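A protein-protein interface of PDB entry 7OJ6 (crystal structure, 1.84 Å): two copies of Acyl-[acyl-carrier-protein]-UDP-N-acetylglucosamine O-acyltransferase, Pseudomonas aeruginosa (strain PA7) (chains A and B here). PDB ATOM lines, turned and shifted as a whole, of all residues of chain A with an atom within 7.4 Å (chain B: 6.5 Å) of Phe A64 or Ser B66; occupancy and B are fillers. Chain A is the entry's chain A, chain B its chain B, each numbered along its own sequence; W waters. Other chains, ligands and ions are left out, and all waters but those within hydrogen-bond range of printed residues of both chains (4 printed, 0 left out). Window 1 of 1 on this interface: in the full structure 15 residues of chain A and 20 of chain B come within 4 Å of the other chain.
His A46 touches His B46. O of His B46 touches CZ of Phe A64, at 3.3 Å. Phe A64 touches Phe B64. Phe A64 touches Ser B66. Arg A92 touches His B98. OE2 of Glu A93 touches CG2 of Thr B96, 3.1 Å away. O of Phe B64 touches OH of Tyr A119, 3.8 Å away. Tyr A119 touches Thr B96.
Printed residues of chain A that touch a printed residue of chain B: His A46, Gln A63, Phe A64, Arg A92, Glu A93 and Tyr A119. Hydrophobic or aromatic side chains of chain A that line the printed part of chain B: His A46, Phe A64 and Tyr A119. Hydrophobic or aromatic side chains of chain B within 4 Å of the printed part of chain A: His B46, Phe B64 and His B98.
Water W2 bridges OH of Tyr A119 (2.4 Å) and O of Phe B64 (3.0 Å). Water W1 lies within hydrogen-bond range of the side-chain carboxylate (OE2) of Glu A93 (2.7 Å) and a ring nitrogen (NE2) of His B98 (2.8 Å). Water W3 lies within hydrogen-bond range of the side-chain carboxylate (OE1) of Glu B69 (2.8 Å) and the side-chain amide nitrogen (NE2) of Gln A63 (3.1 Å). Water W4 lies within hydrogen-bond range of the backbone carbonyl oxygen (O) of Phe B64, the side-chain hydroxyl (OG) of Ser B66 and the side-chain hydroxyl (OH) of Tyr A119.
Of chain B, only His B46 (3.3 Å), Phe B64 (3.4 Å) and Ser B66 (3.7 Å) come within 4 Å of Phe A64. Printed residues of chain A within 4 Å of His B98: Arg A92 (3.9 Å). Printed residues of chain B within 4 Å of Gln A63: Ser B66 and Glu B69. Printed residues of chain A within 4 Å of Gly B94: Tyr A119. Printed residues of chain B within 4 Å of His A46: His B46 (3.0 Å). Of the printed residues of chain A, His B46 touches His A46 (3.0 Å) and Phe A64 (3.3 Å). Val B47 touches none of the printed residues of chain A. Pro A45 touches none of the printed residues of chain B.
The guanidinium group (NH2) of Arg A92 is in salt-bridge range of the side-chain carboxylate (OE1) of Glu B69. The side-chain amide nitrogen of Gln A63 sits at hydrogen-bond distance from the side-chain hydroxyl of Ser B66 (3.1 Å). The side-chain hydroxyl of Tyr A119 lies within hydrogen-bond range of the backbone carbonyl oxygen of Gly B94 (2.9 Å). OE1 of Glu B69 lies within hydrogen-bond range of NE2 of Gln A63 (3.5 Å). The side-chain carboxylate (OE2) of Glu B69 sits close to the side-chain carboxylate (OE2) of Glu A93, at 2.7 Å.
The side-chain carboxylate (OE1) of Glu A93 is in salt-bridge range of the guanidinium group (NH2) of Arg A92. OG of Ser B65 lies within hydrogen-bond range of N of Gly B94, at 3.5 Å. The side-chain hydroxyl (OG) of Ser A65 is in hydrogen-bond range of the backbone carbonyl oxygen (O) of Arg A92 (2.9 Å). N of Phe A64 lies within hydrogen-bond range of O of His A46 (2.8 Å). N of Glu B69 is in hydrogen-bond range of O of Ile B97. The backbone NH (N) of Ser B66 lies within hydrogen-bond range of the backbone carbonyl oxygen (O) of Val B95 (2.9 Å).
Gln A63 touches Ser B66, but with the chains exchanged Ser A66 does not touch Gln B63 (13.7 Å). Phe A64 touches His B46, but with the chains exchanged His A46 does not touch Phe B64 (6.1 Å). Phe B64 touches its own counterpart, Phe A64. Phe A64 touches Ser B66, but with the chains exchanged Ser A66 does not touch Phe B64 (10.2 Å). Positions printed for both chains: 46, 47, 48, 62, 63, 64, 65, 66, 67, 94, 95 and 96. Of the 13 pairs that touch across the chains among the printed residues, 2 have their exchanged pair printed and touching as well.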
ATOM      1  N   SER A  29     -28.838  -2.658  14.640  1.00  0.00           N
ATOM      2  CA  SER A  29     -29.414  -1.589  13.853  1.00  0.00           C
ATOM      3  C   SER A  29     -30.993  -1.558  14.047  1.00  0.00           C
ATOM      4  O   SER A  29     -31.601  -2.605  14.333  1.00  0.00           O
ATOM      5  CB  SER A  29     -29.140  -1.779  12.376  1.00  0.00           C
ATOM      6  OG  SER A  29     -27.752  -1.402  12.132  1.00  0.00           O
ATOM      7  N   GLY A  44     -25.635  -1.120   7.518  1.00  0.00           N
ATOM      8  CA  GLY A  44     -24.561  -1.670   8.366  1.00  0.00           C
ATOM      9  C   GLY A  44     -25.093  -1.932   9.763  1.00  0.00           C
ATOM     10  O   GLY A  44     -26.285  -1.894  10.048  1.00  0.00           O
ATOM     11  N   PRO A  45     -24.124  -2.156  10.698  1.00  0.00           N
ATOM     12  CA  PRO A  45     -24.434  -2.330  12.096  1.00  0.00           C
ATOM     13  C   PRO A  45     -24.572  -0.965  12.760  1.00  0.00           C
ATOM     14  O   PRO A  45     -24.054   0.022  12.300  1.00  0.00           O
ATOM     15  CB  PRO A  45     -23.183  -3.105  12.653  1.00  0.00           C
ATOM     16  CG  PRO A  45     -22.040  -2.541  11.795  1.00  0.00           C
ATOM     17  CD  PRO A  45     -22.654  -2.268  10.428  1.00  0.00           C
ATOM     18  N   HIS A  46     -25.242  -0.912  13.918  1.00  0.00           N
ATOM     19  CA  HIS A  46     -25.270   0.294  14.723  1.00  0.00           C
ATOM     20  C   HIS A  46     -25.887   1.473  13.923  1.00  0.00           C
ATOM     21  O   HIS A  46     -25.457   2.634  14.087  1.00  0.00           O
ATOM     22  CB  HIS A  46     -23.889   0.713  15.262  1.00  0.00           C
ATOM     23  CG  HIS A  46     -23.297  -0.242  16.159  1.00  0.00           C
ATOM     24  ND1 HIS A  46     -23.856  -0.480  17.354  1.00  0.00           N
ATOM     25  CD2 HIS A  46     -22.156  -0.974  16.107  1.00  0.00           C
ATOM     26  CE1 HIS A  46     -23.113  -1.350  18.004  1.00  0.00           C
ATOM     27  NE2 HIS A  46     -22.068  -1.629  17.274  1.00  0.00           N
ATOM     28  N   VAL A  47     -26.892   1.200  13.054  1.00  0.00           N
ATOM     29  CA  VAL A  47     -27.500   2.282  12.250  1.00  0.00           C
ATOM     30  C   VAL A  47     -28.882   2.584  12.899  1.00  0.00           C
ATOM     31  O   VAL A  47     -29.579   1.625  13.277  1.00  0.00           O
ATOM     32  CB  VAL A  47     -27.666   1.923  10.817  1.00  0.00           C
ATOM     33  CG1 VAL A  47     -28.432   2.990  10.031  1.00  0.00           C
ATOM     34  CG2 VAL A  47     -26.293   1.807  10.141  1.00  0.00           C
ATOM     35  N   VAL A  48     -29.264   3.868  12.975  1.00  0.00           N
ATOM     36  CA  VAL A  48     -30.600   4.226  13.431  1.00  0.00           C
ATOM     37  C   VAL A  48     -31.369   4.850  12.207  1.00  0.00           C
ATOM     38  O   VAL A  48     -30.924   5.879  11.699  1.00  0.00           O
ATOM     39  CB  VAL A  48     -30.561   5.238  14.556  1.00  0.00           C
ATOM     40  CG1 VAL A  48     -32.063   5.600  15.044  1.00  0.00           C
ATOM     41  CG2 VAL A  48     -29.943   4.579  15.805  1.00  0.00           C
ATOM     42  N   ILE A  61     -25.485   2.249   3.886  1.00  0.00           N
ATOM     43  CA  ILE A  61     -25.486   3.142   5.019  1.00  0.00           C
ATOM     44  C   ILE A  61     -24.657   2.496   6.160  1.00  0.00           C
ATOM     45  O   ILE A  61     -24.912   1.411   6.557  1.00  0.00           O
ATOM     46  CB  ILE A  61     -26.945   3.375   5.460  1.00  0.00           C
ATOM     47  CG1 ILE A  61     -27.804   3.946   4.273  1.00  0.00           C
ATOM     48  CG2 ILE A  61     -26.990   4.348   6.606  1.00  0.00           C
ATOM     49  CD1 ILE A  61     -29.168   4.347   4.744  1.00  0.00           C
ATOM     50  N   TYR A  62     -23.619   3.226   6.581  1.00  0.00           N
ATOM     51  CA  TYR A  62     -22.584   2.755   7.472  1.00  0.00           C
ATOM     52  C   TYR A  62     -22.960   3.116   8.950  1.00  0.00           C
ATOM     53  O   TYR A  62     -23.869   3.906   9.231  1.00  0.00           O
ATOM     54  CB  TYR A  62     -21.251   3.374   7.107  1.00  0.00           C
ATOM     55  CG  TYR A  62     -20.569   2.676   5.955  1.00  0.00           C
ATOM     56  CD1 TYR A  62     -20.940   2.983   4.629  1.00  0.00           C
ATOM     57  CD2 TYR A  62     -19.505   1.782   6.155  1.00  0.00           C
ATOM     58  CE1 TYR A  62     -20.397   2.286   3.574  1.00  0.00           C
ATOM     59  CE2 TYR A  62     -18.892   1.133   5.120  1.00  0.00           C
ATOM     60  CZ  TYR A  62     -19.364   1.478   3.783  1.00  0.00           C
ATOM     61  OH  TYR A  62     -18.789   0.866   2.690  1.00  0.00           O
ATOM     62  N   GLN A  63     -22.284   2.404   9.823  1.00  0.00           N
ATOM     63  CA  GLN A  63     -22.377   2.517  11.263  1.00  0.00           C
ATOM     64  C   GLN A  63     -22.482   3.905  11.849  1.00  0.00           C
ATOM     65  O   GLN A  63     -21.751   4.802  11.448  1.00  0.00           O
ATOM     66  CB  GLN A  63     -21.307   1.740  11.951  1.00  0.00           C
ATOM     67  CG  GLN A  63     -19.874   2.235  11.608  1.00  0.00           C
ATOM     68  CD  GLN A  63     -19.242   1.419  10.474  1.00  0.00           C
ATOM     69  OE1 GLN A  63     -19.913   0.766   9.674  1.00  0.00           O
ATOM     70  NE2 GLN A  63     -17.937   1.619  10.315  1.00  0.00           N
ATOM     71  N   PHE A  64     -23.364   4.005  12.851  1.00  0.00           N
ATOM     72  CA  PHE A  64     -23.413   5.169  13.764  1.00  0.00           C
ATOM     73  C   PHE A  64     -24.071   6.349  13.067  1.00  0.00           C
ATOM     74  O   PHE A  64     -24.077   7.460  13.588  1.00  0.00           O
ATOM     75  CB  PHE A  64     -22.044   5.607  14.335  1.00  0.00           C
ATOM     76  CG  PHE A  64     -21.228   4.473  14.873  1.00  0.00           C
ATOM     77  CD1 PHE A  64     -21.741   3.552  15.760  1.00  0.00           C
ATOM     78  CD2 PHE A  64     -19.917   4.266  14.422  1.00  0.00           C
ATOM     79  CE1 PHE A  64     -20.997   2.485  16.304  1.00  0.00           C
ATOM     80  CE2 PHE A  64     -19.213   3.161  14.921  1.00  0.00           C
ATOM     81  CZ  PHE A  64     -19.709   2.322  15.835  1.00  0.00           C
ATOM     82  N   SER A  65     -24.714   6.114  11.972  1.00  0.00           N
ATOM     83  CA  SER A  65     -25.495   7.082  11.169  1.00  0.00           C
ATOM     84  C   SER A  65     -26.946   7.128  11.755  1.00  0.00           C
ATOM     85  O   SER A  65     -27.428   6.123  12.282  1.00  0.00           O
ATOM     86  CB  SER A  65     -25.727   6.645   9.712  1.00  0.00           C
ATOM     87  OG  SER A  65     -24.482   6.985   9.164  1.00  0.00           O
ATOM     88  N   SER A  66     -27.562   8.330  11.739  1.00  0.00           N
ATOM     89  CA  SER A  66     -28.977   8.552  12.235  1.00  0.00           C
ATOM     90  C   SER A  66     -29.671   9.206  10.960  1.00  0.00           C
ATOM     91  O   SER A  66     -29.404  10.380  10.650  1.00  0.00           O
ATOM     92  CB  SER A  66     -29.070   9.543  13.393  1.00  0.00           C
ATOM     93  OG  SER A  66     -28.431   8.965  14.536  1.00  0.00           O
ATOM     94  N   VAL A  67     -30.454   8.430  10.300  1.00  0.00           N
ATOM     95  CA  VAL A  67     -31.047   8.788   9.041  1.00  0.00           C
ATOM     96  C   VAL A  67     -32.563   8.837   9.198  1.00  0.00           C
ATOM     97  O   VAL A  67     -33.191   7.880   9.582  1.00  0.00           O
ATOM     98  CB  VAL A  67     -30.550   7.831   7.966  1.00  0.00           C
ATOM     99  CG1 VAL A  67     -31.297   8.116   6.622  1.00  0.00           C
ATOM    100  CG2 VAL A  67     -29.069   7.912   7.720  1.00  0.00           C
ATOM    101  N   ARG A  92     -21.823   7.348   4.750  1.00  0.00           N
ATOM    102  CA  ARG A  92     -20.702   6.849   5.568  1.00  0.00           C
ATOM    103  C   ARG A  92     -21.057   6.971   7.043  1.00  0.00           C
ATOM    104  O   ARG A  92     -22.147   7.372   7.444  1.00  0.00           O
ATOM    105  CB  ARG A  92     -19.403   7.628   5.221  1.00  0.00           C
ATOM    106  CG  ARG A  92     -18.887   7.296   3.820  1.00  0.00           C
ATOM    107  CD  ARG A  92     -18.516   5.891   3.456  1.00  0.00           C
ATOM    108  NE  ARG A  92     -17.553   5.545   4.494  1.00  0.00           N
ATOM    109  CZ  ARG A  92     -16.779   4.462   4.498  1.00  0.00           C
ATOM    110  NH1 ARG A  92     -16.751   3.662   3.461  1.00  0.00           N
ATOM    111  NH2 ARG A  92     -15.940   4.263   5.525  1.00  0.00           N
ATOM    112  N   GLU A  93     -20.128   6.637   7.878  1.00  0.00           N
ATOM    113  CA  GLU A  93     -20.396   6.599   9.253  1.00  0.00           C
ATOM    114  C   GLU A  93     -20.718   7.938   9.923  1.00  0.00           C
ATOM    115  O   GLU A  93     -20.158   8.999   9.638  1.00  0.00           O
ATOM    116  CB  GLU A  93     -19.224   5.872   9.994  1.00  0.00           C
ATOM    117  CG  GLU A  93     -17.956   6.440   9.964  1.00  0.00           C
ATOM    118  CD  GLU A  93     -17.052   6.150   8.698  1.00  0.00           C
ATOM    119  OE1 GLU A  93     -17.480   5.849   7.579  1.00  0.00           O
ATOM    120  OE2 GLU A  93     -15.833   6.567   8.853  1.00  0.00           O
ATOM    121  N   GLY A  94     -21.652   7.850  10.882  1.00  0.00           N
ATOM    122  CA  GLY A  94     -21.931   9.027  11.650  1.00  0.00           C
ATOM    123  C   GLY A  94     -22.723  10.133  10.945  1.00  0.00           C
ATOM    124  O   GLY A  94     -22.907  11.157  11.553  1.00  0.00           O
ATOM    125  N   VAL A  95     -23.232   9.881   9.794  1.00  0.00           N
ATOM    126  CA  VAL A  95     -23.969  10.919   9.032  1.00  0.00           C
ATOM    127  C   VAL A  95     -25.337  11.129   9.710  1.00  0.00           C
ATOM    128  O   VAL A  95     -25.963  10.151  10.164  1.00  0.00           O
ATOM    129  CB  VAL A  95     -24.097  10.462   7.612  1.00  0.00           C
ATOM    130  CG1 VAL A  95     -25.166  11.324   6.837  1.00  0.00           C
ATOM    131  CG2 VAL A  95     -22.694  10.616   6.945  1.00  0.00           C
ATOM    132  N   THR A  96     -25.792  12.385   9.819  1.00  0.00           N
ATOM    133  CA  THR A  96     -27.114  12.707  10.299  1.00  0.00           C
ATOM    134  C   THR A  96     -27.923  13.364   9.169  1.00  0.00           C
ATOM    135  O   THR A  96     -27.411  14.320   8.518  1.00  0.00           O
ATOM    136  CB  THR A  96     -27.016  13.636  11.477  1.00  0.00           C
ATOM    137  OG1 THR A  96     -26.202  14.774  11.202  1.00  0.00           O
ATOM    138  CG2 THR A  96     -26.319  12.932  12.663  1.00  0.00           C
ATOM    139  N   TYR A 119     -19.784  11.850   9.163  1.00  0.00           N
ATOM    140  CA  TYR A 119     -20.213  12.877  10.070  1.00  0.00           C
ATOM    141  C   TYR A 119     -20.784  14.055   9.363  1.00  0.00           C
ATOM    142  O   TYR A 119     -20.966  15.121  10.003  1.00  0.00           O
ATOM    143  CB  TYR A 119     -19.124  13.332  11.058  1.00  0.00           C
ATOM    144  CG  TYR A 119     -18.678  12.151  11.925  1.00  0.00           C
ATOM    145  CD1 TYR A 119     -19.535  11.593  12.840  1.00  0.00           C
ATOM    146  CD2 TYR A 119     -17.431  11.506  11.724  1.00  0.00           C
ATOM    147  CE1 TYR A 119     -19.221  10.488  13.624  1.00  0.00           C
ATOM    148  CE2 TYR A 119     -17.106  10.358  12.444  1.00  0.00           C
ATOM    149  CZ  TYR A 119     -18.004   9.807  13.373  1.00  0.00           C
ATOM    150  OH  TYR A 119     -17.628   8.756  14.187  1.00  0.00           O
ATOM    151  N   HIS B  46     -18.971  -0.928  21.297  1.00  0.00           N
ATOM    152  CA  HIS B  46     -19.480  -0.206  20.085  1.00  0.00           C
ATOM    153  C   HIS B  46     -18.287   0.245  19.238  1.00  0.00           C
ATOM    154  O   HIS B  46     -18.366   1.300  18.671  1.00  0.00           O
ATOM    155  CB  HIS B  46     -20.301   1.043  20.503  1.00  0.00           C
ATOM    156  CG  HIS B  46     -21.577   0.715  21.180  1.00  0.00           C
ATOM    157  ND1 HIS B  46     -22.530   0.002  20.607  1.00  0.00           N
ATOM    158  CD2 HIS B  46     -22.072   1.084  22.367  1.00  0.00           C
ATOM    159  CE1 HIS B  46     -23.567  -0.109  21.391  1.00  0.00           C
ATOM    160  NE2 HIS B  46     -23.331   0.631  22.415  1.00  0.00           N
ATOM    161  N   VAL B  47     -17.254  -0.579  19.155  1.00  0.00           N
ATOM    162  CA  VAL B  47     -16.087  -0.276  18.331  1.00  0.00           C
ATOM    163  C   VAL B  47     -16.118  -1.168  17.094  1.00  0.00           C
ATOM    164  O   VAL B  47     -16.517  -2.328  17.168  1.00  0.00           O
ATOM    165  CB  VAL B  47     -14.798  -0.522  19.071  1.00  0.00           C
ATOM    166  CG1 VAL B  47     -13.557  -0.311  18.111  1.00  0.00           C
ATOM    167  CG2 VAL B  47     -14.627   0.426  20.201  1.00  0.00           C
ATOM    168  N   VAL B  48     -15.813  -0.628  15.956  1.00  0.00           N
ATOM    169  CA  VAL B  48     -15.708  -1.427  14.706  1.00  0.00           C
ATOM    170  C   VAL B  48     -14.253  -1.454  14.257  1.00  0.00           C
ATOM    171  O   VAL B  48     -13.716  -0.380  13.945  1.00  0.00           O
ATOM    172  CB  VAL B  48     -16.624  -0.817  13.555  1.00  0.00           C
ATOM    173  CG1 VAL B  48     -16.410  -1.611  12.235  1.00  0.00           C
ATOM    174  CG2 VAL B  48     -18.103  -0.859  13.926  1.00  0.00           C
ATOM    175  N   LEU B  49     -13.631  -2.641  14.223  1.00  0.00           N
ATOM    176  CA  LEU B  49     -12.291  -2.814  13.755  1.00  0.00           C
ATOM    177  C   LEU B  49     -12.341  -3.639  12.484  1.00  0.00           C
ATOM    178  O   LEU B  49     -12.922  -4.716  12.475  1.00  0.00           O
ATOM    179  CB  LEU B  49     -11.400  -3.556  14.762  1.00  0.00           C
ATOM    180  CG  LEU B  49     -11.292  -2.937  16.093  1.00  0.00           C
ATOM    181  CD1 LEU B  49     -10.338  -3.741  17.009  1.00  0.00           C
ATOM    182  CD2 LEU B  49     -10.779  -1.523  16.102  1.00  0.00           C
ATOM    183  N   LYS B  50     -11.710  -3.181  11.416  1.00  0.00           N
ATOM    184  CA  LYS B  50     -11.674  -3.929  10.165  1.00  0.00           C
ATOM    185  C   LYS B  50     -10.219  -3.987   9.737  1.00  0.00           C
ATOM    186  O   LYS B  50      -9.392  -3.211  10.158  1.00  0.00           O
ATOM    187  CB  LYS B  50     -12.601  -3.142   9.192  1.00  0.00           C
ATOM    188  CG  LYS B  50     -12.569  -3.658   7.814  1.00  0.00           C
ATOM    189  CD  LYS B  50     -13.626  -3.011   6.806  1.00  0.00           C
ATOM    190  CE  LYS B  50     -13.735  -3.954   5.559  1.00  0.00           C
ATOM    191  NZ  LYS B  50     -14.759  -3.252   4.782  1.00  0.00           N
ATOM    192  N   TYR B  62     -11.785   3.644  22.142  1.00  0.00           N
ATOM    193  CA  TYR B  62     -13.055   3.965  22.724  1.00  0.00           C
ATOM    194  C   TYR B  62     -14.203   3.893  21.693  1.00  0.00           C
ATOM    195  O   TYR B  62     -13.988   3.754  20.499  1.00  0.00           O
ATOM    196  CB  TYR B  62     -13.034   5.404  23.190  1.00  0.00           C
ATOM    197  CG  TYR B  62     -12.277   5.526  24.531  1.00  0.00           C
ATOM    198  CD1 TYR B  62     -10.912   5.496  24.561  1.00  0.00           C
ATOM    199  CD2 TYR B  62     -12.995   5.717  25.722  1.00  0.00           C
ATOM    200  CE1 TYR B  62     -10.220   5.684  25.792  1.00  0.00           C
ATOM    201  CE2 TYR B  62     -12.363   5.766  26.992  1.00  0.00           C
ATOM    202  CZ  TYR B  62     -10.948   5.857  26.976  1.00  0.00           C
ATOM    203  OH  TYR B  62     -10.245   5.896  28.161  1.00  0.00           O
ATOM    204  N   GLN B  63     -15.404   3.824  22.286  1.00  0.00           N
ATOM    205  CA  GLN B  63     -16.669   3.672  21.690  1.00  0.00           C
ATOM    206  C   GLN B  63     -16.911   4.506  20.435  1.00  0.00           C
ATOM    207  O   GLN B  63     -16.512   5.690  20.366  1.00  0.00           O
ATOM    208  CB  GLN B  63     -17.796   3.917  22.650  1.00  0.00           C
ATOM    209  CG  GLN B  63     -17.908   5.262  23.265  1.00  0.00           C
ATOM    210  CD  GLN B  63     -17.133   5.349  24.631  1.00  0.00           C
ATOM    211  OE1 GLN B  63     -16.364   4.446  24.954  1.00  0.00           O
ATOM    212  NE2 GLN B  63     -17.290   6.430  25.303  1.00  0.00           N
ATOM    213  N   PHE B  64     -17.594   3.890  19.500  1.00  0.00           N
ATOM    214  CA  PHE B  64     -18.043   4.520  18.251  1.00  0.00           C
ATOM    215  C   PHE B  64     -16.961   4.845  17.222  1.00  0.00           C
ATOM    216  O   PHE B  64     -17.216   5.579  16.259  1.00  0.00           O
ATOM    217  CB  PHE B  64     -18.936   5.736  18.496  1.00  0.00           C
ATOM    218  CG  PHE B  64     -19.920   5.520  19.636  1.00  0.00           C
ATOM    219  CD1 PHE B  64     -20.828   4.468  19.638  1.00  0.00           C
ATOM    220  CD2 PHE B  64     -19.965   6.393  20.702  1.00  0.00           C
ATOM    221  CE1 PHE B  64     -21.792   4.260  20.639  1.00  0.00           C
ATOM    222  CE2 PHE B  64     -20.895   6.192  21.746  1.00  0.00           C
ATOM    223  CZ  PHE B  64     -21.769   5.147  21.728  1.00  0.00           C
ATOM    224  N   SER B  65     -15.819   4.379  17.433  1.00  0.00           N
ATOM    225  CA  SER B  65     -14.601   4.466  16.553  1.00  0.00           C
ATOM    226  C   SER B  65     -14.755   3.428  15.416  1.00  0.00           C
ATOM    227  O   SER B  65     -15.260   2.310  15.661  1.00  0.00           O
ATOM    228  CB  SER B  65     -13.328   4.121  17.343  1.00  0.00           C
ATOM    229  OG  SER B  65     -13.134   5.329  17.953  1.00  0.00           O
ATOM    230  N   SER B  66     -14.240   3.749  14.225  1.00  0.00           N
ATOM    231  CA  SER B  66     -14.222   2.858  13.097  1.00  0.00           C
ATOM    232  C   SER B  66     -12.731   2.859  12.662  1.00  0.00           C
ATOM    233  O   SER B  66     -12.248   3.898  12.088  1.00  0.00           O
ATOM    234  CB  SER B  66     -15.096   3.306  11.900  1.00  0.00           C
ATOM    235  OG  SER B  66     -16.489   3.361  12.371  1.00  0.00           O
ATOM    236  N   VAL B  67     -12.055   1.770  12.907  1.00  0.00           N
ATOM    237  CA  VAL B  67     -10.596   1.725  12.748  1.00  0.00           C
ATOM    238  C   VAL B  67     -10.309   0.660  11.807  1.00  0.00           C
ATOM    239  O   VAL B  67     -10.652  -0.532  11.987  1.00  0.00           O
ATOM    240  CB  VAL B  67      -9.953   1.499  14.077  1.00  0.00           C
ATOM    241  CG1 VAL B  67      -8.435   1.269  14.007  1.00  0.00           C
ATOM    242  CG2 VAL B  67     -10.209   2.644  15.067  1.00  0.00           C
ATOM    243  N   GLY B  68      -9.723   1.010  10.727  1.00  0.00           N
ATOM    244  CA  GLY B  68      -9.348   0.037   9.675  1.00  0.00           C
ATOM    245  C   GLY B  68     -10.226   0.018   8.496  1.00  0.00           C
ATOM    246  O   GLY B  68     -10.336  -0.974   7.795  1.00  0.00           O
ATOM    247  N   GLU B  69     -10.885   1.150   8.237  1.00  0.00           N
ATOM    248  CA  GLU B  69     -11.811   1.248   7.101  1.00  0.00           C
ATOM    249  C   GLU B  69     -11.115   1.309   5.764  1.00  0.00           C
ATOM    250  O   GLU B  69      -9.943   1.674   5.624  1.00  0.00           O
ATOM    251  CB  GLU B  69     -12.497   2.584   7.218  1.00  0.00           C
ATOM    252  CG  GLU B  69     -13.082   2.685   8.655  1.00  0.00           C
ATOM    253  CD  GLU B  69     -14.215   3.627   8.616  1.00  0.00           C
ATOM    254  OE1 GLU B  69     -15.418   3.074   8.443  1.00  0.00           O
ATOM    255  OE2 GLU B  69     -13.742   4.855   8.727  1.00  0.00           O
ATOM    256  N   GLY B  94     -15.385   7.882  18.541  1.00  0.00           N
ATOM    257  CA  GLY B  94     -15.812   8.408  17.206  1.00  0.00           C
ATOM    258  C   GLY B  94     -14.641   8.571  16.169  1.00  0.00           C
ATOM    259  O   GLY B  94     -14.933   9.118  15.084  1.00  0.00           O
ATOM    260  N   VAL B  95     -13.469   8.186  16.483  1.00  0.00           N
ATOM    261  CA  VAL B  95     -12.340   8.355  15.577  1.00  0.00           C
ATOM    262  C   VAL B  95     -12.486   7.464  14.343  1.00  0.00           C
ATOM    263  O   VAL B  95     -12.948   6.329  14.473  1.00  0.00           O
ATOM    264  CB  VAL B  95     -11.026   8.078  16.296  1.00  0.00           C
ATOM    265  CG1 VAL B  95      -9.783   7.957  15.325  1.00  0.00           C
ATOM    266  CG2 VAL B  95     -10.834   9.280  17.306  1.00  0.00           C
ATOM    267  N   THR B  96     -12.127   7.984  13.189  1.00  0.00           N
ATOM    268  CA  THR B  96     -12.122   7.191  11.936  1.00  0.00           C
ATOM    269  C   THR B  96     -10.688   7.102  11.436  1.00  0.00           C
ATOM    270  O   THR B  96     -10.039   8.147  11.298  1.00  0.00           O
ATOM    271  CB  THR B  96     -13.072   7.784  10.878  1.00  0.00           C
ATOM    272  OG1 THR B  96     -12.807   9.213  10.693  1.00  0.00           O
ATOM    273  CG2 THR B  96     -14.551   7.692  11.392  1.00  0.00           C
ATOM    274  N   ILE B  97     -10.221   5.907  11.130  1.00  0.00           N
ATOM    275  CA  ILE B  97      -8.872   5.648  10.567  1.00  0.00           C
ATOM    276  C   ILE B  97      -8.964   4.734   9.435  1.00  0.00           C
ATOM    277  O   ILE B  97      -9.510   3.616   9.542  1.00  0.00           O
ATOM    278  CB  ILE B  97      -7.954   5.104  11.672  1.00  0.00           C
ATOM    279  CG1 ILE B  97      -8.041   5.930  12.932  1.00  0.00           C
ATOM    280  CG2 ILE B  97      -6.484   4.934  11.160  1.00  0.00           C
ATOM    281  CD1 ILE B  97      -7.130   5.395  14.105  1.00  0.00           C
ATOM    282  N   HIS B  98      -8.488   5.135   8.251  1.00  0.00           N
ATOM    283  CA  HIS B  98      -8.556   4.293   7.074  1.00  0.00           C
ATOM    284  C   HIS B  98      -7.220   3.599   6.839  1.00  0.00           C
ATOM    285  O   HIS B  98      -6.138   4.118   7.211  1.00  0.00           O
ATOM    286  CB  HIS B  98      -8.903   5.172   5.875  1.00  0.00           C
ATOM    287  CG  HIS B  98     -10.295   5.680   5.921  1.00  0.00           C
ATOM    288  ND1 HIS B  98     -11.237   5.271   5.027  1.00  0.00           N
ATOM    289  CD2 HIS B  98     -10.977   6.371   6.859  1.00  0.00           C
ATOM    290  CE1 HIS B  98     -12.366   5.915   5.254  1.00  0.00           C
ATOM    291  NE2 HIS B  98     -12.265   6.518   6.397  1.00  0.00           N
HETATM  292  O   HOH W   1     -14.170   8.205   7.541  1.00  0.00           O
HETATM  293  O   HOH W   2     -19.320   7.445  15.336  1.00  0.00           O
HETATM  294  O   HOH W   3     -16.264   0.490   8.009  1.00  0.00           O
HETATM  295  O   HOH W   4     -16.865   5.851  13.538  1.00  0.00           O
